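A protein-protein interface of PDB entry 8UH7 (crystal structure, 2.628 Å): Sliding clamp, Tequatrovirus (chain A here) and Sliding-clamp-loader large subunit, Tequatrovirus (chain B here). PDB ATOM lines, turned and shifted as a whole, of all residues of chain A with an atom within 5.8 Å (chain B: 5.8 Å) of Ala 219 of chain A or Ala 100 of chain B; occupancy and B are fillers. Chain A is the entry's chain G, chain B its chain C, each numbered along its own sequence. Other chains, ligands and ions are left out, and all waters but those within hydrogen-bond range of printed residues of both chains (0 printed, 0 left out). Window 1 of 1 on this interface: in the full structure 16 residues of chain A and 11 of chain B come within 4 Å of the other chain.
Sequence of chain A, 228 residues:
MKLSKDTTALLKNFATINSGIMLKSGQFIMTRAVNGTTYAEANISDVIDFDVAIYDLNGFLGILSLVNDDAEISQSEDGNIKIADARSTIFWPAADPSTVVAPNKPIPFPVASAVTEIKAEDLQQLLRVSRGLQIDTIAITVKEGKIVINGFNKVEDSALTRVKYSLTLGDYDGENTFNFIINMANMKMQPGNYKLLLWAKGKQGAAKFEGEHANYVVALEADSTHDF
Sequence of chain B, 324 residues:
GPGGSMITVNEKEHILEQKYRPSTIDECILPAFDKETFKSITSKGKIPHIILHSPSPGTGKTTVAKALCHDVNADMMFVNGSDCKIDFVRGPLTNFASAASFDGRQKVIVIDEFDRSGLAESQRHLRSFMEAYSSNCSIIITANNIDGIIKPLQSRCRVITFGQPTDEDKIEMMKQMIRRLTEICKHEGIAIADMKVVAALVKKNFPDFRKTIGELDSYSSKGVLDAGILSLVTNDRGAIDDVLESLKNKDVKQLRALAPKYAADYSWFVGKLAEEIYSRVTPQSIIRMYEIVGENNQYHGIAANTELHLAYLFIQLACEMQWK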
ATOM      1  N   GLY A  36      24.941   1.753 -22.133  1.00  0.00           N
ATOM      2  CA  GLY A  36      23.649   2.334 -22.462  1.00  0.00           C
ATOM      3  C   GLY A  36      22.463   1.641 -21.830  1.00  0.00           C
ATOM      4  O   GLY A  36      21.417   1.491 -22.474  1.00  0.00           O
ATOM      5  N   THR A  37      22.602   1.205 -20.582  1.00  0.00           N
ATOM      6  CA  THR A  37      21.508   0.553 -19.876  1.00  0.00           C
ATOM      7  C   THR A  37      20.767   1.490 -18.934  1.00  0.00           C
ATOM      8  O   THR A  37      19.537   1.433 -18.855  1.00  0.00           O
ATOM      9  CB  THR A  37      22.024  -0.657 -19.088  1.00  0.00           C
ATOM     10  OG1 THR A  37      23.281  -0.336 -18.478  1.00  0.00           O
ATOM     11  CG2 THR A  37      22.192  -1.858 -20.006  1.00  0.00           C
ATOM     12  N   THR A  38      21.482   2.352 -18.213  1.00  0.00           N
ATOM     13  CA  THR A  38      20.861   3.309 -17.311  1.00  0.00           C
ATOM     14  C   THR A  38      21.407   4.704 -17.581  1.00  0.00           C
ATOM     15  O   THR A  38      22.566   4.877 -17.968  1.00  0.00           O
ATOM     16  CB  THR A  38      21.084   2.942 -15.829  1.00  0.00           C
ATOM     17  OG1 THR A  38      22.105   3.780 -15.274  1.00  0.00           O
ATOM     18  CG2 THR A  38      21.504   1.485 -15.683  1.00  0.00           C
ATOM     19  N   ILE A 181       9.905  -6.198 -18.515  1.00  0.00           N
ATOM     20  CA  ILE A 181      10.941  -6.877 -17.751  1.00  0.00           C
ATOM     21  C   ILE A 181      12.119  -5.926 -17.587  1.00  0.00           C
ATOM     22  O   ILE A 181      12.527  -5.251 -18.540  1.00  0.00           O
ATOM     23  CB  ILE A 181      11.373  -8.179 -18.443  1.00  0.00           C
ATOM     24  CG1 ILE A 181      10.145  -8.973 -18.894  1.00  0.00           C
ATOM     25  CG2 ILE A 181      12.244  -9.013 -17.512  1.00  0.00           C
ATOM     26  CD1 ILE A 181      10.479 -10.169 -19.758  1.00  0.00           C
ATOM     27  N   ILE A 182      12.656  -5.861 -16.373  1.00  0.00           N
ATOM     28  CA  ILE A 182      13.789  -5.007 -16.051  1.00  0.00           C
ATOM     29  C   ILE A 182      14.798  -5.832 -15.265  1.00  0.00           C
ATOM     30  O   ILE A 182      14.429  -6.546 -14.323  1.00  0.00           O
ATOM     31  CB  ILE A 182      13.365  -3.756 -15.253  1.00  0.00           C
ATOM     32  CG1 ILE A 182      12.376  -2.912 -16.059  1.00  0.00           C
ATOM     33  CG2 ILE A 182      14.573  -2.909 -14.891  1.00  0.00           C
ATOM     34  CD1 ILE A 182      12.023  -1.599 -15.396  1.00  0.00           C
ATOM     35  N   ASN A 183      16.064  -5.745 -15.664  1.00  0.00           N
ATOM     36  CA  ASN A 183      17.145  -6.414 -14.956  1.00  0.00           C
ATOM     37  C   ASN A 183      17.515  -5.611 -13.716  1.00  0.00           C
ATOM     38  O   ASN A 183      17.709  -4.393 -13.791  1.00  0.00           O
ATOM     39  CB  ASN A 183      18.355  -6.574 -15.876  1.00  0.00           C
ATOM     40  CG  ASN A 183      19.523  -7.254 -15.193  1.00  0.00           C
ATOM     41  OD1 ASN A 183      19.344  -8.056 -14.277  1.00  0.00           O
ATOM     42  ND2 ASN A 183      20.732  -6.936 -15.641  1.00  0.00           N
ATOM     43  N   ASN A 186      20.408  -2.905 -13.377  1.00  0.00           N
ATOM     44  CA  ASN A 186      20.276  -1.560 -13.920  1.00  0.00           C
ATOM     45  C   ASN A 186      19.509  -0.617 -12.998  1.00  0.00           C
ATOM     46  O   ASN A 186      19.252   0.530 -13.381  1.00  0.00           O
ATOM     47  CB  ASN A 186      19.605  -1.619 -15.293  1.00  0.00           C
ATOM     48  CG  ASN A 186      20.432  -2.384 -16.308  1.00  0.00           C
ATOM     49  OD1 ASN A 186      21.663  -2.351 -16.273  1.00  0.00           O
ATOM     50  ND2 ASN A 186      19.761  -3.082 -17.217  1.00  0.00           N
ATOM     51  N   LYS A 203       8.981  -1.850 -30.871  1.00  0.00           N
ATOM     52  CA  LYS A 203      10.313  -2.315 -30.509  1.00  0.00           C
ATOM     53  C   LYS A 203      11.006  -1.420 -29.490  1.00  0.00           C
ATOM     54  O   LYS A 203      11.909  -1.889 -28.790  1.00  0.00           O
ATOM     55  CB  LYS A 203      11.177  -2.425 -31.768  1.00  0.00           C
ATOM     56  CG  LYS A 203      10.913  -1.317 -32.782  1.00  0.00           C
ATOM     57  CD  LYS A 203      11.276  -1.749 -34.193  1.00  0.00           C
ATOM     58  CE  LYS A 203      10.655  -0.820 -35.225  1.00  0.00           C
ATOM     59  NZ  LYS A 203       9.167  -0.797 -35.129  1.00  0.00           N
ATOM     60  N   GLY A 205      11.343   1.127 -26.094  1.00  0.00           N
ATOM     61  CA  GLY A 205      10.777   1.180 -24.758  1.00  0.00           C
ATOM     62  C   GLY A 205      11.793   1.664 -23.746  1.00  0.00           C
ATOM     63  O   GLY A 205      13.006   1.618 -23.974  1.00  0.00           O
ATOM     64  N   ALA A 206      11.266   2.121 -22.612  1.00  0.00           N
ATOM     65  CA  ALA A 206      12.087   2.625 -21.517  1.00  0.00           C
ATOM     66  C   ALA A 206      11.214   2.809 -20.282  1.00  0.00           C
ATOM     67  O   ALA A 206       9.981   2.878 -20.373  1.00  0.00           O
ATOM     68  CB  ALA A 206      12.774   3.944 -21.889  1.00  0.00           C
ATOM     69  N   ALA A 207      11.873   2.893 -19.124  1.00  0.00           N
ATOM     70  CA  ALA A 207      11.199   3.118 -17.850  1.00  0.00           C
ATOM     71  C   ALA A 207      11.885   4.265 -17.123  1.00  0.00           C
ATOM     72  O   ALA A 207      13.068   4.166 -16.788  1.00  0.00           O
ATOM     73  CB  ALA A 207      11.214   1.853 -16.987  1.00  0.00           C
ATOM     74  N   VAL A 217      16.485   6.939 -16.075  1.00  0.00           N
ATOM     75  CA  VAL A 217      15.953   6.198 -17.211  1.00  0.00           C
ATOM     76  C   VAL A 217      16.627   4.834 -17.247  1.00  0.00           C
ATOM     77  O   VAL A 217      17.851   4.736 -17.110  1.00  0.00           O
ATOM     78  CB  VAL A 217      16.175   6.960 -18.527  1.00  0.00           C
ATOM     79  CG1 VAL A 217      15.561   6.196 -19.694  1.00  0.00           C
ATOM     80  CG2 VAL A 217      15.594   8.359 -18.427  1.00  0.00           C
ATOM     81  N   VAL A 218      15.834   3.781 -17.426  1.00  0.00           N
ATOM     82  CA  VAL A 218      16.325   2.409 -17.420  1.00  0.00           C
ATOM     83  C   VAL A 218      15.805   1.705 -18.664  1.00  0.00           C
ATOM     84  O   VAL A 218      14.624   1.837 -19.014  1.00  0.00           O
ATOM     85  CB  VAL A 218      15.892   1.655 -16.148  1.00  0.00           C
ATOM     86  CG1 VAL A 218      16.335   0.203 -16.207  1.00  0.00           C
ATOM     87  CG2 VAL A 218      16.456   2.335 -14.911  1.00  0.00           C
ATOM     88  N   ALA A 219      16.687   0.968 -19.334  1.00  0.00           N
ATOM     89  CA  ALA A 219      16.301   0.187 -20.499  1.00  0.00           C
ATOM     90  C   ALA A 219      15.630  -1.107 -20.068  1.00  0.00           C
ATOM     91  O   ALA A 219      16.026  -1.734 -19.082  1.00  0.00           O
ATOM     92  CB  ALA A 219      17.519  -0.121 -21.370  1.00  0.00           C
ATOM     93  N   LEU A 220      14.606  -1.501 -20.814  1.00  0.00           N
ATOM     94  CA  LEU A 220      13.885  -2.728 -20.523  1.00  0.00           C
ATOM     95  C   LEU A 220      14.615  -3.922 -21.128  1.00  0.00           C
ATOM     96  O   LEU A 220      15.488  -3.780 -21.988  1.00  0.00           O
ATOM     97  CB  LEU A 220      12.463  -2.644 -21.070  1.00  0.00           C
ATOM     98  CG  LEU A 220      11.887  -1.228 -21.031  1.00  0.00           C
ATOM     99  CD1 LEU A 220      10.679  -1.124 -21.936  1.00  0.00           C
ATOM    100  CD2 LEU A 220      11.537  -0.824 -19.605  1.00  0.00           C
ATOM    101  N   GLU A 221      14.247  -5.113 -20.665  1.00  0.00           N
ATOM    102  CA  GLU A 221      14.838  -6.326 -21.208  1.00  0.00           C
ATOM    103  C   GLU A 221      14.270  -6.617 -22.592  1.00  0.00           C
ATOM    104  O   GLU A 221      13.158  -6.203 -22.933  1.00  0.00           O
ATOM    105  CB  GLU A 221      14.604  -7.504 -20.267  1.00  0.00           C
ATOM    106  CG  GLU A 221      15.198  -7.282 -18.888  1.00  0.00           C
ATOM    107  CD  GLU A 221      16.642  -6.806 -18.946  1.00  0.00           C
ATOM    108  OE1 GLU A 221      17.524  -7.613 -19.304  1.00  0.00           O
ATOM    109  OE2 GLU A 221      16.893  -5.619 -18.645  1.00  0.00           O
ATOM    110  N   ALA A 222      15.056  -7.336 -23.395  1.00  0.00           N
ATOM    111  CA  ALA A 222      14.732  -7.493 -24.811  1.00  0.00           C
ATOM    112  C   ALA A 222      13.392  -8.189 -25.008  1.00  0.00           C
ATOM    113  O   ALA A 222      12.634  -7.843 -25.922  1.00  0.00           O
ATOM    114  CB  ALA A 222      15.846  -8.264 -25.519  1.00  0.00           C
ATOM    115  N   PHE B  96      24.263  -5.585 -21.575  1.00  0.00           N
ATOM    116  CA  PHE B  96      24.004  -4.977 -22.873  1.00  0.00           C
ATOM    117  C   PHE B  96      23.264  -5.938 -23.794  1.00  0.00           C
ATOM    118  O   PHE B  96      22.317  -5.539 -24.481  1.00  0.00           O
ATOM    119  CB  PHE B  96      25.322  -4.528 -23.499  1.00  0.00           C
ATOM    120  CG  PHE B  96      25.177  -3.913 -24.861  1.00  0.00           C
ATOM    121  CD1 PHE B  96      24.755  -2.601 -25.003  1.00  0.00           C
ATOM    122  CD2 PHE B  96      25.484  -4.640 -25.999  1.00  0.00           C
ATOM    123  CE1 PHE B  96      24.627  -2.031 -26.257  1.00  0.00           C
ATOM    124  CE2 PHE B  96      25.359  -4.074 -27.256  1.00  0.00           C
ATOM    125  CZ  PHE B  96      24.930  -2.769 -27.384  1.00  0.00           C
ATOM    126  N   SER B  98      21.347  -8.575 -23.008  1.00  0.00           N
ATOM    127  CA  SER B  98      20.015  -8.963 -22.557  1.00  0.00           C
ATOM    128  C   SER B  98      19.031  -7.802 -22.605  1.00  0.00           C
ATOM    129  O   SER B  98      17.833  -8.022 -22.819  1.00  0.00           O
ATOM    130  CB  SER B  98      20.082  -9.530 -21.138  1.00  0.00           C
ATOM    131  OG  SER B  98      20.488  -8.542 -20.209  1.00  0.00           O
ATOM    132  N   ALA B  99      19.507  -6.576 -22.412  1.00  0.00           N
ATOM    133  CA  ALA B  99      18.641  -5.410 -22.436  1.00  0.00           C
ATOM    134  C   ALA B  99      18.303  -5.015 -23.871  1.00  0.00           C
ATOM    135  O   ALA B  99      18.987  -5.390 -24.827  1.00  0.00           O
ATOM    136  CB  ALA B  99      19.297  -4.233 -21.713  1.00  0.00           C
ATOM    137  N   ALA B 100      17.229  -4.247 -24.008  1.00  0.00           N
ATOM    138  CA  ALA B 100      16.782  -3.748 -25.298  1.00  0.00           C
ATOM    139  C   ALA B 100      17.261  -2.317 -25.511  1.00  0.00           C
ATOM    140  O   ALA B 100      17.546  -1.582 -24.563  1.00  0.00           O
ATOM    141  CB  ALA B 100      15.256  -3.810 -25.405  1.00  0.00           C
ATOM    142  N   SER B 101      17.359  -1.934 -26.779  1.00  0.00           N
ATOM    143  CA  SER B 101      17.731  -0.572 -27.123  1.00  0.00           C
ATOM    144  C   SER B 101      16.517   0.340 -26.998  1.00  0.00           C
ATOM    145  O   SER B 101      15.388  -0.065 -27.288  1.00  0.00           O
ATOM    146  CB  SER B 101      18.297  -0.513 -28.542  1.00  0.00           C
ATOM    147  OG  SER B 101      17.372  -1.034 -29.480  1.00  0.00           O
ATOM    148  N   PHE B 102      16.758   1.577 -26.558  1.00  0.00           N
ATOM    149  CA  PHE B 102      15.665   2.521 -26.356  1.00  0.00           C
ATOM    150  C   PHE B 102      14.948   2.870 -27.654  1.00  0.00           C
ATOM    151  O   PHE B 102      13.811   3.351 -27.607  1.00  0.00           O
ATOM    152  CB  PHE B 102      16.179   3.807 -25.707  1.00  0.00           C
ATOM    153  CG  PHE B 102      16.951   3.590 -24.436  1.00  0.00           C
ATOM    154  CD1 PHE B 102      16.295   3.446 -23.225  1.00  0.00           C
ATOM    155  CD2 PHE B 102      18.338   3.551 -24.449  1.00  0.00           C
ATOM    156  CE1 PHE B 102      17.004   3.258 -22.053  1.00  0.00           C
ATOM    157  CE2 PHE B 102      19.052   3.362 -23.281  1.00  0.00           C
ATOM    158  CZ  PHE B 102      18.385   3.215 -22.082  1.00  0.00           C
ATOM    159  N   LYS B 107      21.391  -4.507 -31.322  1.00  0.00           N
ATOM    160  CA  LYS B 107      22.615  -4.338 -30.555  1.00  0.00           C
ATOM    161  C   LYS B 107      23.709  -5.239 -31.113  1.00  0.00           C
ATOM    162  O   LYS B 107      23.470  -6.411 -31.423  1.00  0.00           O
ATOM    163  CB  LYS B 107      22.371  -4.648 -29.079  1.00  0.00           C
ATOM    164  CG  LYS B 107      21.506  -3.615 -28.366  1.00  0.00           C
ATOM    165  CD  LYS B 107      21.198  -4.051 -26.945  1.00  0.00           C
ATOM    166  CE  LYS B 107      20.574  -2.934 -26.126  1.00  0.00           C
ATOM    167  NZ  LYS B 107      21.515  -1.807 -25.879  1.00  0.00           N
ATOM    168  N   ASN B 136      18.739 -11.001 -29.727  1.00  0.00           N
ATOM    169  CA  ASN B 136      18.796  -9.556 -29.544  1.00  0.00           C
ATOM    170  C   ASN B 136      20.134  -8.944 -29.923  1.00  0.00           C
ATOM    171  O   ASN B 136      20.162  -7.855 -30.501  1.00  0.00           O
ATOM    172  CB  ASN B 136      18.481  -9.202 -28.085  1.00  0.00           C
ATOM    173  CG  ASN B 136      18.565  -7.710 -27.810  1.00  0.00           C
ATOM    174  OD1 ASN B 136      18.275  -6.886 -28.678  1.00  0.00           O
ATOM    175  ND2 ASN B 136      18.965  -7.358 -26.594  1.00  0.00           N
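Ala 219 of chain A touches just these residues of chain B: Ala 100 (3.5 Å) and Phe 102 (3.5 Å). Of chain A, only Ala 219 (3.5 Å), Leu 220 (2.7 Å) and Ala 222 (3.8 Å) come within 4 Å of Ala 100 of chain B. Of the printed residues of chain A, Ser 98 of chain B touches Glu 221 (3.2 Å) and Ala 222 (2.9 Å). Printed residues of chain B within 4 Å of Gly 205 of chain A: Phe 102. Of the printed residues of chain A, Ala 99 of chain B touches Leu 220 and Glu 221. Of the printed residues of chain B, Ala 206 of chain A touches Phe 102 (3.8 Å). Ile 181 of chain A touches none of the printed residues of chain B. Ala 207 of chain A touches none of the printed residues of chain B. The nearest residue of chain A that does not touch Ala 100 of chain B is Glu 221 of chain A (4.03 Å). The nearest printed residue of chain A that does not touch Phe 102 of chain B is Val 217 of chain A (4.03 Å).
OE1 of Glu 221 of chain A sits at hydrogen-bond distance from OG of Ser 98 of chain B, at 3.2 Å. O of Ser 98 of chain B is in hydrogen-bond range of N of Ala 222 of chain A (2.9 Å). N of Ala 100 of chain B lies within hydrogen-bond range of O of Leu 220 of chain A (2.7 Å).
Among the printed residues, merely in contact across the chains: Gly 36 of chain A with Phe 102 of chain B, Thr 37 of chain A with Phe 102 of chain B, Gly 205 of chain A with Phe 102 of chain B, Ala 206 of chain A with Phe 102 of chain B, Val 218 of chain A with Phe 102 of chain B, Ala 219 of chain A with Ala 100 of chain B, Ala 219 of chain A with Phe 102 of chain B, Leu 220 of chain A with Ala 99 of chain B, Glu 221 of chain A with Ala 99 of chain B, Ala 222 of chain A with Ala 100 of chain B and Ala 222 of chain A with Asn 136 of chain B.
Of the 17 printed residues of chain A, 9 touch a printed residue of chain B. Of the 8 printed residues of chain B, 5 touch a printed residue of chain A. Printed residues of chain B that touch a printed residue of chain A: Ser 98, Ala 99, Ala 100, Phe 102 and Asn 136. Hydrophobic or aromatic side chains of chain B that line the printed part of chain A: Ala 99, Ala 100 and Phe 102. Among the printed residues, no Asp or Glu carboxylate lies within 4 Å of a Lys or Arg side-chain nitrogen of the other chain.
O of Ala 207 of chain A lies within hydrogen-bond range of N of Val 218 of chain A, 2.9 Å away. O of Ala 99 of chain B sits at hydrogen-bond distance from ND2 of Asn 136 of chain B. The backbone carbonyl oxygen (O) of Ile 181 of chain A lies within hydrogen-bond range of the backbone NH (N) of Glu 221 of chain A, 2.7 Å away. The backbone carbonyl oxygen of Thr 37 of chain A sits at hydrogen-bond distance from the backbone NH of Ala 219 of chain A (2.9 Å). The side-chain amide oxygen (OD1) of Asn 186 of chain A sits close to the side-chain hydroxyl (OG1) of Thr 37 of chain A (3.4 Å). The side-chain carboxylate (OE2) of Glu 221 of chain A sits at hydrogen-bond distance from the backbone NH (N) of Asn 183 of chain A.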
